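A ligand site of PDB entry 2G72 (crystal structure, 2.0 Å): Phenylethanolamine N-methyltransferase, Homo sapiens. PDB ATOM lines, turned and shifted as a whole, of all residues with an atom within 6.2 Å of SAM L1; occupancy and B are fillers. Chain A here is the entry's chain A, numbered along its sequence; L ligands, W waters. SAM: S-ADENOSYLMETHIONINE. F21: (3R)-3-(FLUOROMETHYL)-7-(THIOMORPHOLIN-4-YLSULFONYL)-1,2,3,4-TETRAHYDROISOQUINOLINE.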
ATOM      1  N   VAL A  23      -8.979 -25.459  14.981  1.00  0.00           N
ATOM      2  CA  VAL A  23     -10.415 -25.446  15.242  1.00  0.00           C
ATOM      3  C   VAL A  23     -10.619 -26.188  16.562  1.00  0.00           C
ATOM      4  O   VAL A  23     -11.284 -25.692  17.472  1.00  0.00           O
ATOM      5  CB  VAL A  23     -11.208 -26.162  14.115  1.00  0.00           C
ATOM      6  CG1 VAL A  23     -12.658 -26.356  14.512  1.00  0.00           C
ATOM      7  CG2 VAL A  23     -11.123 -25.353  12.815  1.00  0.00           C
ATOM      8  N   ALA A  24     -10.028 -27.374  16.642  1.00  0.00           N
ATOM      9  CA  ALA A  24     -10.119 -28.222  17.831  1.00  0.00           C
ATOM     10  C   ALA A  24      -9.767 -27.448  19.094  1.00  0.00           C
ATOM     11  O   ALA A  24     -10.309 -27.707  20.175  1.00  0.00           O
ATOM     12  CB  ALA A  24      -9.181 -29.434  17.682  1.00  0.00           C
ATOM     13  N   TYR A  27     -12.689 -25.010  19.995  1.00  0.00           N
ATOM     14  CA  TYR A  27     -13.805 -25.722  20.601  1.00  0.00           C
ATOM     15  C   TYR A  27     -13.599 -26.121  22.055  1.00  0.00           C
ATOM     16  O   TYR A  27     -14.548 -26.496  22.740  1.00  0.00           O
ATOM     17  CB  TYR A  27     -14.180 -26.949  19.774  1.00  0.00           C
ATOM     18  CG  TYR A  27     -15.137 -26.607  18.655  1.00  0.00           C
ATOM     19  CD1 TYR A  27     -14.668 -26.333  17.380  1.00  0.00           C
ATOM     20  CD2 TYR A  27     -16.506 -26.444  18.905  1.00  0.00           C
ATOM     21  CE1 TYR A  27     -15.539 -25.916  16.377  1.00  0.00           C
ATOM     22  CE2 TYR A  27     -17.377 -26.026  17.902  1.00  0.00           C
ATOM     23  CZ  TYR A  27     -16.887 -25.771  16.652  1.00  0.00           C
ATOM     24  OH  TYR A  27     -17.739 -25.333  15.666  1.00  0.00           O
ATOM     25  N   PHE A  30     -15.800 -23.961  24.055  1.00  0.00           N
ATOM     26  CA  PHE A  30     -17.235 -24.030  23.726  1.00  0.00           C
ATOM     27  C   PHE A  30     -18.126 -24.320  24.935  1.00  0.00           C
ATOM     28  O   PHE A  30     -18.053 -25.388  25.543  1.00  0.00           O
ATOM     29  CB  PHE A  30     -17.449 -25.108  22.653  1.00  0.00           C
ATOM     30  CG  PHE A  30     -18.872 -25.269  22.210  1.00  0.00           C
ATOM     31  CD1 PHE A  30     -19.311 -24.707  21.008  1.00  0.00           C
ATOM     32  CD2 PHE A  30     -19.779 -26.001  22.972  1.00  0.00           C
ATOM     33  CE1 PHE A  30     -20.614 -24.882  20.565  1.00  0.00           C
ATOM     34  CE2 PHE A  30     -21.097 -26.194  22.545  1.00  0.00           C
ATOM     35  CZ  PHE A  30     -21.518 -25.632  21.336  1.00  0.00           C
ATOM     36  N   TYR A  35     -24.368 -21.705  24.147  1.00  0.00           N
ATOM     37  CA  TYR A  35     -24.770 -22.037  22.780  1.00  0.00           C
ATOM     38  C   TYR A  35     -26.290 -22.212  22.690  1.00  0.00           C
ATOM     39  O   TYR A  35     -26.950 -21.675  21.784  1.00  0.00           O
ATOM     40  CB  TYR A  35     -24.071 -23.323  22.317  1.00  0.00           C
ATOM     41  CG  TYR A  35     -24.514 -23.797  20.943  1.00  0.00           C
ATOM     42  CD1 TYR A  35     -24.080 -23.147  19.783  1.00  0.00           C
ATOM     43  CD2 TYR A  35     -25.372 -24.886  20.799  1.00  0.00           C
ATOM     44  CE1 TYR A  35     -24.491 -23.575  18.529  1.00  0.00           C
ATOM     45  CE2 TYR A  35     -25.789 -25.331  19.532  1.00  0.00           C
ATOM     46  CZ  TYR A  35     -25.336 -24.660  18.414  1.00  0.00           C
ATOM     47  OH  TYR A  35     -25.752 -25.061  17.172  1.00  0.00           O
ATOM     48  N   TYR A  40     -31.242 -21.558  20.774  1.00  0.00           N
ATOM     49  CA  TYR A  40     -32.503 -22.240  20.971  1.00  0.00           C
ATOM     50  C   TYR A  40     -33.495 -21.623  21.921  1.00  0.00           C
ATOM     51  O   TYR A  40     -34.593 -22.133  22.076  1.00  0.00           O
ATOM     52  CB  TYR A  40     -32.229 -23.719  21.249  1.00  0.00           C
ATOM     53  CG  TYR A  40     -31.526 -24.330  20.064  1.00  0.00           C
ATOM     54  CD1 TYR A  40     -30.130 -24.326  19.983  1.00  0.00           C
ATOM     55  CD2 TYR A  40     -32.239 -24.809  18.973  1.00  0.00           C
ATOM     56  CE1 TYR A  40     -29.462 -24.775  18.852  1.00  0.00           C
ATOM     57  CE2 TYR A  40     -31.601 -25.261  17.847  1.00  0.00           C
ATOM     58  CZ  TYR A  40     -30.213 -25.243  17.774  1.00  0.00           C
ATOM     59  OH  TYR A  40     -29.569 -25.677  16.635  1.00  0.00           O
ATOM     60  N   ASP A  77     -26.695 -39.315  14.111  1.00  0.00           N
ATOM     61  CA  ASP A  77     -26.773 -37.862  14.133  1.00  0.00           C
ATOM     62  C   ASP A  77     -25.342 -37.393  14.319  1.00  0.00           C
ATOM     63  O   ASP A  77     -24.736 -37.629  15.375  1.00  0.00           O
ATOM     64  CB  ASP A  77     -27.674 -37.376  15.278  1.00  0.00           C
ATOM     65  CG  ASP A  77     -27.782 -35.850  15.325  1.00  0.00           C
ATOM     66  OD1 ASP A  77     -27.815 -35.226  14.246  1.00  0.00           O
ATOM     67  OD2 ASP A  77     -27.836 -35.276  16.425  1.00  0.00           O
ATOM     68  N   ILE A  78     -24.827 -36.717  13.291  1.00  0.00           N
ATOM     69  CA  ILE A  78     -23.449 -36.211  13.229  1.00  0.00           C
ATOM     70  C   ILE A  78     -23.279 -34.821  13.823  1.00  0.00           C
ATOM     71  O   ILE A  78     -23.805 -33.837  13.283  1.00  0.00           O
ATOM     72  CB  ILE A  78     -22.945 -36.111  11.748  1.00  0.00           C
ATOM     73  CG1 ILE A  78     -23.190 -37.416  10.974  1.00  0.00           C
ATOM     74  CG2 ILE A  78     -21.493 -35.672  11.734  1.00  0.00           C
ATOM     75  CD1 ILE A  78     -22.522 -38.665  11.537  1.00  0.00           C
ATOM     76  N   GLY A  79     -22.505 -34.720  14.885  1.00  0.00           N
ATOM     77  CA  GLY A  79     -22.275 -33.421  15.499  1.00  0.00           C
ATOM     78  C   GLY A  79     -23.529 -32.906  16.184  1.00  0.00           C
ATOM     79  O   GLY A  79     -23.931 -31.763  15.966  1.00  0.00           O
ATOM     80  N   SER A  80     -24.119 -33.751  17.030  1.00  0.00           N
ATOM     81  CA  SER A  80     -25.325 -33.427  17.766  1.00  0.00           C
ATOM     82  C   SER A  80     -25.202 -32.217  18.668  1.00  0.00           C
ATOM     83  O   SER A  80     -26.186 -31.515  18.905  1.00  0.00           O
ATOM     84  CB  SER A  80     -25.734 -34.611  18.654  1.00  0.00           C
ATOM     85  OG  SER A  80     -25.881 -35.795  17.895  1.00  0.00           O
ATOM     86  N   GLY A  81     -24.005 -31.980  19.188  1.00  0.00           N
ATOM     87  CA  GLY A  81     -23.840 -30.862  20.118  1.00  0.00           C
ATOM     88  C   GLY A  81     -24.776 -31.150  21.298  1.00  0.00           C
ATOM     89  O   GLY A  81     -24.954 -32.306  21.666  1.00  0.00           O
ATOM     90  N   PRO A  82     -25.382 -30.120  21.898  1.00  0.00           N
ATOM     91  CA  PRO A  82     -26.283 -30.346  23.030  1.00  0.00           C
ATOM     92  C   PRO A  82     -27.744 -30.242  22.626  1.00  0.00           C
ATOM     93  O   PRO A  82     -28.600 -29.876  23.435  1.00  0.00           O
ATOM     94  CB  PRO A  82     -25.902 -29.220  23.978  1.00  0.00           C
ATOM     95  CG  PRO A  82     -25.744 -28.072  22.994  1.00  0.00           C
ATOM     96  CD  PRO A  82     -25.038 -28.692  21.788  1.00  0.00           C
ATOM     97  N   THR A  83     -28.065 -30.557  21.369  1.00  0.00           N
ATOM     98  CA  THR A  83     -29.440 -30.421  20.934  1.00  0.00           C
ATOM     99  C   THR A  83     -30.066 -31.717  20.463  1.00  0.00           C
ATOM    100  O   THR A  83     -29.370 -32.614  20.009  1.00  0.00           O
ATOM    101  CB  THR A  83     -29.554 -29.345  19.807  1.00  0.00           C
ATOM    102  OG1 THR A  83     -29.116 -29.871  18.555  1.00  0.00           O
ATOM    103  CG2 THR A  83     -28.669 -28.161  20.132  1.00  0.00           C
ATOM    104  N   TYR A  85     -33.531 -31.383  18.978  1.00  0.00           N
ATOM    105  CA  TYR A  85     -34.655 -31.006  18.098  1.00  0.00           C
ATOM    106  C   TYR A  85     -34.518 -31.625  16.716  1.00  0.00           C
ATOM    107  O   TYR A  85     -35.536 -31.958  16.090  1.00  0.00           O
ATOM    108  CB  TYR A  85     -34.749 -29.496  17.953  1.00  0.00           C
ATOM    109  CG  TYR A  85     -33.709 -28.942  17.014  1.00  0.00           C
ATOM    110  CD1 TYR A  85     -33.958 -28.847  15.637  1.00  0.00           C
ATOM    111  CD2 TYR A  85     -32.423 -28.627  17.479  1.00  0.00           C
ATOM    112  CE1 TYR A  85     -32.942 -28.449  14.753  1.00  0.00           C
ATOM    113  CE2 TYR A  85     -31.401 -28.244  16.611  1.00  0.00           C
ATOM    114  CZ  TYR A  85     -31.671 -28.161  15.238  1.00  0.00           C
ATOM    115  OH  TYR A  85     -30.652 -27.845  14.393  1.00  0.00           O
ATOM    116  N   GLN A  86     -33.290 -31.766  16.239  1.00  0.00           N
ATOM    117  CA  GLN A  86     -33.036 -32.328  14.920  1.00  0.00           C
ATOM    118  C   GLN A  86     -33.502 -33.775  14.804  1.00  0.00           C
ATOM    119  O   GLN A  86     -33.590 -34.308  13.698  1.00  0.00           O
ATOM    120  CB  GLN A  86     -31.547 -32.208  14.519  1.00  0.00           C
ATOM    121  CG  GLN A  86     -30.560 -33.058  15.326  1.00  0.00           C
ATOM    122  CD  GLN A  86     -30.089 -32.383  16.596  1.00  0.00           C
ATOM    123  OE1 GLN A  86     -30.756 -31.506  17.144  1.00  0.00           O
ATOM    124  NE2 GLN A  86     -28.936 -32.802  17.095  1.00  0.00           N
ATOM    125  N   THR A 100     -23.914 -38.138  18.373  1.00  0.00           N
ATOM    126  CA  THR A 100     -22.483 -37.977  18.487  1.00  0.00           C
ATOM    127  C   THR A 100     -22.006 -36.549  18.631  1.00  0.00           C
ATOM    128  O   THR A 100     -22.704 -35.610  18.277  1.00  0.00           O
ATOM    129  CB  THR A 100     -21.761 -38.525  17.237  1.00  0.00           C
ATOM    130  OG1 THR A 100     -22.162 -37.750  16.104  1.00  0.00           O
ATOM    131  CG2 THR A 100     -22.109 -39.988  16.991  1.00  0.00           C
ATOM    132  N   ASP A 101     -20.798 -36.406  19.183  1.00  0.00           N
ATOM    133  CA  ASP A 101     -20.148 -35.124  19.287  1.00  0.00           C
ATOM    134  C   ASP A 101     -18.691 -35.201  19.703  1.00  0.00           C
ATOM    135  O   ASP A 101     -18.275 -36.075  20.456  1.00  0.00           O
ATOM    136  CB  ASP A 101     -20.871 -34.173  20.198  1.00  0.00           C
ATOM    137  CG  ASP A 101     -20.559 -32.728  19.864  1.00  0.00           C
ATOM    138  OD1 ASP A 101     -21.063 -32.249  18.820  1.00  0.00           O
ATOM    139  OD2 ASP A 101     -19.795 -32.094  20.610  1.00  0.00           O
ATOM    140  N   PHE A 102     -17.920 -34.238  19.187  1.00  0.00           N
ATOM    141  CA  PHE A 102     -16.503 -34.137  19.447  1.00  0.00           C
ATOM    142  C   PHE A 102     -16.187 -33.775  20.887  1.00  0.00           C
ATOM    143  O   PHE A 102     -15.198 -34.250  21.442  1.00  0.00           O
ATOM    144  CB  PHE A 102     -15.928 -33.075  18.522  1.00  0.00           C
ATOM    145  CG  PHE A 102     -14.449 -32.903  18.619  1.00  0.00           C
ATOM    146  CD1 PHE A 102     -13.583 -33.865  18.109  1.00  0.00           C
ATOM    147  CD2 PHE A 102     -13.916 -31.775  19.243  1.00  0.00           C
ATOM    148  CE1 PHE A 102     -12.200 -33.716  18.213  1.00  0.00           C
ATOM    149  CE2 PHE A 102     -12.530 -31.612  19.351  1.00  0.00           C
ATOM    150  CZ  PHE A 102     -11.677 -32.578  18.837  1.00  0.00           C
ATOM    151  N   LEU A 103     -17.027 -32.955  21.518  1.00  0.00           N
ATOM    152  CA  LEU A 103     -16.772 -32.522  22.890  1.00  0.00           C
ATOM    153  C   LEU A 103     -17.433 -33.363  23.972  1.00  0.00           C
ATOM    154  O   LEU A 103     -18.570 -33.809  23.809  1.00  0.00           O
ATOM    155  CB  LEU A 103     -17.202 -31.060  23.080  1.00  0.00           C
ATOM    156  CG  LEU A 103     -16.531 -30.061  22.155  1.00  0.00           C
ATOM    157  CD1 LEU A 103     -17.010 -28.643  22.462  1.00  0.00           C
ATOM    158  CD2 LEU A 103     -15.021 -30.173  22.323  1.00  0.00           C
ATOM    159  N   ASN A 106     -20.592 -31.618  25.614  1.00  0.00           N
ATOM    160  CA  ASN A 106     -21.849 -31.698  24.895  1.00  0.00           C
ATOM    161  C   ASN A 106     -22.485 -33.062  25.129  1.00  0.00           C
ATOM    162  O   ASN A 106     -23.701 -33.151  25.354  1.00  0.00           O
ATOM    163  CB  ASN A 106     -21.662 -31.486  23.405  1.00  0.00           C
ATOM    164  CG  ASN A 106     -21.579 -30.021  23.044  1.00  0.00           C
ATOM    165  OD1 ASN A 106     -22.253 -29.194  23.657  1.00  0.00           O
ATOM    166  ND2 ASN A 106     -20.753 -29.708  22.059  1.00  0.00           N
ATOM    167  N   ILE A 157     -16.751 -38.313  18.163  1.00  0.00           N
ATOM    168  CA  ILE A 157     -16.620 -38.377  16.718  1.00  0.00           C
ATOM    169  C   ILE A 157     -15.742 -37.209  16.255  1.00  0.00           C
ATOM    170  O   ILE A 157     -15.586 -36.217  16.975  1.00  0.00           O
ATOM    171  CB  ILE A 157     -18.033 -38.303  16.053  1.00  0.00           C
ATOM    172  CG1 ILE A 157     -17.938 -38.426  14.534  1.00  0.00           C
ATOM    173  CG2 ILE A 157     -18.736 -36.988  16.430  1.00  0.00           C
ATOM    174  CD1 ILE A 157     -19.305 -38.524  13.838  1.00  0.00           C
ATOM    175  N   ASP A 158     -15.150 -37.371  15.075  1.00  0.00           N
ATOM    176  CA  ASP A 158     -14.306 -36.348  14.470  1.00  0.00           C
ATOM    177  C   ASP A 158     -14.485 -36.482  12.973  1.00  0.00           C
ATOM    178  O   ASP A 158     -13.894 -37.359  12.351  1.00  0.00           O
ATOM    179  CB  ASP A 158     -12.834 -36.567  14.783  1.00  0.00           C
ATOM    180  CG  ASP A 158     -11.965 -35.421  14.299  1.00  0.00           C
ATOM    181  OD1 ASP A 158     -12.375 -34.742  13.328  1.00  0.00           O
ATOM    182  OD2 ASP A 158     -10.867 -35.221  14.871  1.00  0.00           O
ATOM    183  N   VAL A 159     -15.294 -35.603  12.396  1.00  0.00           N
ATOM    184  CA  VAL A 159     -15.563 -35.658  10.985  1.00  0.00           C
ATOM    185  C   VAL A 159     -14.297 -35.478  10.145  1.00  0.00           C
ATOM    186  O   VAL A 159     -14.302 -35.726   8.929  1.00  0.00           O
ATOM    187  CB  VAL A 159     -16.616 -34.596  10.584  1.00  0.00           C
ATOM    188  CG1 VAL A 159     -17.916 -34.845  11.353  1.00  0.00           C
ATOM    189  CG2 VAL A 159     -16.076 -33.204  10.876  1.00  0.00           C
ATOM    190  N   HIS A 160     -13.215 -35.063  10.785  1.00  0.00           N
ATOM    191  CA  HIS A 160     -11.972 -34.856  10.039  1.00  0.00           C
ATOM    192  C   HIS A 160     -11.181 -36.136   9.810  1.00  0.00           C
ATOM    193  O   HIS A 160     -10.300 -36.176   8.956  1.00  0.00           O
ATOM    194  CB  HIS A 160     -11.120 -33.796  10.722  1.00  0.00           C
ATOM    195  CG  HIS A 160     -11.739 -32.439  10.688  1.00  0.00           C
ATOM    196  ND1 HIS A 160     -12.317 -31.916   9.546  1.00  0.00           N
ATOM    197  CD2 HIS A 160     -11.895 -31.500  11.650  1.00  0.00           C
ATOM    198  CE1 HIS A 160     -12.798 -30.712   9.818  1.00  0.00           C
ATOM    199  NE2 HIS A 160     -12.552 -30.439  11.081  1.00  0.00           N
ATOM    200  N   SER A 180     -27.323 -34.271  10.069  1.00  0.00           N
ATOM    201  CA  SER A 180     -26.248 -33.406  10.555  1.00  0.00           C
ATOM    202  C   SER A 180     -26.671 -31.945  10.463  1.00  0.00           C
ATOM    203  O   SER A 180     -26.963 -31.431   9.377  1.00  0.00           O
ATOM    204  CB  SER A 180     -24.962 -33.640   9.772  1.00  0.00           C
ATOM    205  OG  SER A 180     -23.881 -32.960  10.411  1.00  0.00           O
ATOM    206  N   ALA A 181     -26.683 -31.270  11.603  1.00  0.00           N
ATOM    207  CA  ALA A 181     -27.099 -29.878  11.604  1.00  0.00           C
ATOM    208  C   ALA A 181     -26.039 -28.955  12.152  1.00  0.00           C
ATOM    209  O   ALA A 181     -25.611 -29.104  13.293  1.00  0.00           O
ATOM    210  CB  ALA A 181     -28.409 -29.734  12.418  1.00  0.00           C
ATOM    211  N   PHE A 182     -25.611 -28.005  11.326  1.00  0.00           N
ATOM    212  CA  PHE A 182     -24.607 -27.028  11.740  1.00  0.00           C
ATOM    213  C   PHE A 182     -23.269 -27.589  12.227  1.00  0.00           C
ATOM    214  O   PHE A 182     -22.616 -26.997  13.094  1.00  0.00           O
ATOM    215  CB  PHE A 182     -25.181 -26.122  12.824  1.00  0.00           C
ATOM    216  CG  PHE A 182     -26.457 -25.449  12.445  1.00  0.00           C
ATOM    217  CD1 PHE A 182     -27.664 -25.869  12.992  1.00  0.00           C
ATOM    218  CD2 PHE A 182     -26.450 -24.376  11.544  1.00  0.00           C
ATOM    219  CE1 PHE A 182     -28.878 -25.222  12.658  1.00  0.00           C
ATOM    220  CE2 PHE A 182     -27.665 -23.720  11.206  1.00  0.00           C
ATOM    221  CZ  PHE A 182     -28.880 -24.149  11.761  1.00  0.00           C
ATOM    222  N   CYS A 183     -22.851 -28.723  11.682  1.00  0.00           N
ATOM    223  CA  CYS A 183     -21.587 -29.293  12.099  1.00  0.00           C
ATOM    224  C   CYS A 183     -20.450 -29.025  11.104  1.00  0.00           C
ATOM    225  O   CYS A 183     -19.524 -28.263  11.383  1.00  0.00           O
ATOM    226  CB  CYS A 183     -21.729 -30.803  12.303  1.00  0.00           C
ATOM    227  SG  CYS A 183     -20.169 -31.584  12.789  1.00  0.00           S
ATOM    228  N   ALA A 186     -19.238 -25.591  10.460  1.00  0.00           N
ATOM    229  CA  ALA A 186     -18.819 -24.985  11.716  1.00  0.00           C
ATOM    230  C   ALA A 186     -17.511 -25.527  12.281  1.00  0.00           C
ATOM    231  O   ALA A 186     -17.000 -25.030  13.284  1.00  0.00           O
ATOM    232  CB  ALA A 186     -19.914 -25.121  12.770  1.00  0.00           C
ATOM    233  N   VAL A 187     -16.975 -26.572  11.648  1.00  0.00           N
ATOM    234  CA  VAL A 187     -15.724 -27.178  12.113  1.00  0.00           C
ATOM    235  C   VAL A 187     -14.689 -27.257  10.991  1.00  0.00           C
ATOM    236  O   VAL A 187     -13.612 -27.803  11.178  1.00  0.00           O
ATOM    237  CB  VAL A 187     -15.984 -28.598  12.689  1.00  0.00           C
ATOM    238  CG1 VAL A 187     -17.161 -28.560  13.667  1.00  0.00           C
ATOM    239  CG2 VAL A 187     -16.287 -29.573  11.580  1.00  0.00           C
ATOM    240  N   TYR A 222     -19.317 -17.419  15.150  1.00  0.00           N
ATOM    241  CA  TYR A 222     -20.413 -17.483  16.094  1.00  0.00           C
ATOM    242  C   TYR A 222     -19.780 -17.657  17.458  1.00  0.00           C
ATOM    243  O   TYR A 222     -18.650 -18.133  17.560  1.00  0.00           O
ATOM    244  CB  TYR A 222     -21.369 -18.651  15.781  1.00  0.00           C
ATOM    245  CG  TYR A 222     -20.878 -20.025  16.173  1.00  0.00           C
ATOM    246  CD1 TYR A 222     -21.264 -20.588  17.387  1.00  0.00           C
ATOM    247  CD2 TYR A 222     -20.087 -20.782  15.301  1.00  0.00           C
ATOM    248  CE1 TYR A 222     -20.877 -21.876  17.734  1.00  0.00           C
ATOM    249  CE2 TYR A 222     -19.692 -22.083  15.640  1.00  0.00           C
ATOM    250  CZ  TYR A 222     -20.108 -22.627  16.858  1.00  0.00           C
ATOM    251  OH  TYR A 222     -19.755 -23.900  17.201  1.00  0.00           O
HETATM  252  N   SAM L   1     -26.085 -30.130  15.669  1.00  0.00           N
HETATM  253  CA  SAM L   1     -26.248 -29.157  16.737  1.00  0.00           C
HETATM  254  C   SAM L   1     -27.266 -28.087  16.340  1.00  0.00           C
HETATM  255  O   SAM L   1     -28.071 -28.372  15.423  1.00  0.00           O
HETATM  256  OXT SAM L   1     -27.292 -27.002  16.962  1.00  0.00           O
HETATM  257  CB  SAM L   1     -24.887 -28.544  17.124  1.00  0.00           C
HETATM  258  CG  SAM L   1     -24.123 -27.780  16.034  1.00  0.00           C
HETATM  259  SD  SAM L   1     -22.647 -26.890  16.712  1.00  0.00           S
HETATM  260  CE  SAM L   1     -22.643 -25.195  16.125  1.00  0.00           C
HETATM  261  C5' SAM L   1     -21.092 -27.705  16.116  1.00  0.00           C
HETATM  262  C4' SAM L   1     -20.825 -29.033  16.792  1.00  0.00           C
HETATM  263  O4' SAM L   1     -19.723 -29.762  16.177  1.00  0.00           O
HETATM  264  C3' SAM L   1     -20.456 -28.835  18.268  1.00  0.00           C
HETATM  265  O3' SAM L   1     -21.263 -29.657  19.091  1.00  0.00           O
HETATM  266  C2' SAM L   1     -18.980 -29.208  18.305  1.00  0.00           C
HETATM  267  O2' SAM L   1     -18.567 -29.725  19.544  1.00  0.00           O
HETATM  268  C1' SAM L   1     -18.889 -30.263  17.203  1.00  0.00           C
HETATM  269  N9  SAM L   1     -17.544 -30.484  16.653  1.00  0.00           N
HETATM  270  C8  SAM L   1     -16.364 -29.713  16.837  1.00  0.00           C
HETATM  271  N7  SAM L   1     -15.322 -30.211  16.215  1.00  0.00           N
HETATM  272  C5  SAM L   1     -15.819 -31.342  15.601  1.00  0.00           C
HETATM  273  C6  SAM L   1     -15.138 -32.287  14.791  1.00  0.00           C
HETATM  274  N6  SAM L   1     -13.848 -32.209  14.489  1.00  0.00           N
HETATM  275  N1  SAM L   1     -15.872 -33.333  14.302  1.00  0.00           N
HETATM  276  C2  SAM L   1     -17.195 -33.405  14.627  1.00  0.00           C
HETATM  277  N3  SAM L   1     -17.933 -32.555  15.391  1.00  0.00           N
HETATM  278  C4  SAM L   1     -17.173 -31.533  15.843  1.00  0.00           C
HETATM  279  C12 F21 L   2     -32.449 -23.536  13.985  1.00  0.00           C
HETATM  280  C13 F21 L   2     -33.859 -24.130  14.084  1.00  0.00           C
HETATM  281  S2  F21 L   2     -34.370 -24.091  15.835  1.00  0.00           S
HETATM  282  C15 F21 L   2     -33.971 -22.400  16.403  1.00  0.00           C
HETATM  283  C14 F21 L   2     -32.542 -22.071  15.946  1.00  0.00           C
HETATM  284  N1  F21 L   2     -32.500 -22.148  14.476  1.00  0.00           N
HETATM  285  S1  F21 L   2     -31.298 -21.234  13.874  1.00  0.00           S
HETATM  286  O2  F21 L   2     -31.477 -21.177  12.460  1.00  0.00           O
HETATM  287  O1  F21 L   2     -31.449 -19.842  14.433  1.00  0.00           O
HETATM  288  C7  F21 L   2     -29.653 -21.717  14.205  1.00  0.00           C
HETATM  289  C8  F21 L   2     -28.624 -20.900  13.743  1.00  0.00           C
HETATM  290  C9  F21 L   2     -27.291 -21.211  13.996  1.00  0.00           C
HETATM  291  C1  F21 L   2     -26.183 -20.360  13.360  1.00  0.00           C
HETATM  292  N2  F21 L   2     -24.845 -20.666  13.899  1.00  0.00           N
HETATM  293  C3  F21 L   2     -24.616 -22.110  14.047  1.00  0.00           C
HETATM  294  C11 F21 L   2     -23.174 -22.406  14.473  1.00  0.00           C
HETATM  295  F1  F21 L   2     -22.366 -22.454  13.352  1.00  0.00           F
HETATM  296  C4  F21 L   2     -25.549 -22.693  15.109  1.00  0.00           C
HETATM  297  C10 F21 L   2     -26.995 -22.348  14.744  1.00  0.00           C
HETATM  298  C5  F21 L   2     -28.024 -23.174  15.211  1.00  0.00           C
HETATM  299  C6  F21 L   2     -29.351 -22.867  14.945  1.00  0.00           C
HETATM  300  O   HOH W   1     -26.567 -32.783  14.320  1.00  0.00           O
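The side-chain hydroxyl (OH) of Tyr 35 lies within hydrogen-bond range of an oxygen (OXT) of SAM L1 (2.5 Å). The side-chain carboxylate (OD1) of Asp 101 is in hydrogen-bond range of an oxygen (O3') of SAM L1 (2.6 Å). N of SAM L1 is in hydrogen-bond range of O of Ala 181, 2.6 Å away. The side-chain hydroxyl (OH) of Tyr 40 lies within hydrogen-bond range of an oxygen (OXT) of SAM L1 (2.7 Å). O of Gly 79 lies within hydrogen-bond range of N of SAM L1 (2.7 Å). The side-chain hydroxyl of Tyr 85 is in hydrogen-bond range of an oxygen (O) of SAM L1, at 2.8 Å. ND2 of Asn 106 sits at hydrogen-bond distance from O3' of SAM L1 (3.0 Å). N1 of SAM L1 lies within hydrogen-bond range of N of Val 159, at 3.0 Å. N6 of SAM L1 is in hydrogen-bond range of OD1 of Asp 158 (3.2 Å). The side-chain sulfur (SG) of Cys 183 is in hydrogen-bond range of a nitrogen (N3) of SAM L1 (3.6 Å).
SD of SAM L1 sits close to O of Phe 182. CE2 of Tyr 27 touches C2' of SAM L1 (3.6 Å). O of Ser 80 touches CA of SAM L1 (3.2 Å). Gly 81 touches SAM L1 (CA to O3', 3.0 Å). OG1 of Thr 83 touches C of SAM L1 (3.4 Å). CB of Phe 102 touches C4 of SAM L1, at 3.3 Å. CG of Leu 103 touches O2' of SAM L1, 3.3 Å away. Ile 157 touches SAM L1 (O to N1, 3.9 Å). His 160 touches SAM L1 (CD2 to N6, 3.5 Å). Val 187 touches SAM L1 (CG1 to C8, 3.5 Å). Tyr 222 touches SAM L1 (OH to CE, 3.3 Å). Hydrophobic or aromatic side chains that line SAM L1: Tyr 27, Tyr 35, Tyr 40, Tyr 85, Phe 102, Leu 103, Val 159, His 160, Ala 181, Phe 182, Val 187 and Tyr 222. 21 residues have an atom within 4 Å of SAM L1: Tyr 27, Tyr 35, Tyr 40, Gly 79, Ser 80, Gly 81, Thr 83, Tyr 85, Asp 101, Phe 102, Leu 103, Asn 106, Ile 157, Asp 158, Val 159, His 160, Ala 181, Phe 182, Cys 183, Val 187 and Tyr 222. The nearest printed residue that does not touch SAM L1 is Gln 86 (4.2 Å).
OD2 of Asp 101 is in hydrogen-bond range of ND2 of Asn 106 (3.0 Å). The side-chain carboxylate of Asp 101 sits at hydrogen-bond distance from the backbone NH of Gly 81. N of Leu 103 sits at hydrogen-bond distance from OD2 of Asp 101 (3.0 Å). OH of Tyr 40 sits close to OH of Tyr 85. The side-chain carboxylate of Asp 158 sits at hydrogen-bond distance from the backbone NH of His 160. The backbone NH (N) of Ser 80 sits at hydrogen-bond distance from the backbone carbonyl oxygen (O) of Thr 100, at 2.6 Å. The backbone carbonyl oxygen of Val 187 lies within hydrogen-bond range of a ring nitrogen (NE2) of His 160, at 2.8 Å. OH of Tyr 27 sits at hydrogen-bond distance from O of Ala 186 (2.5 Å).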
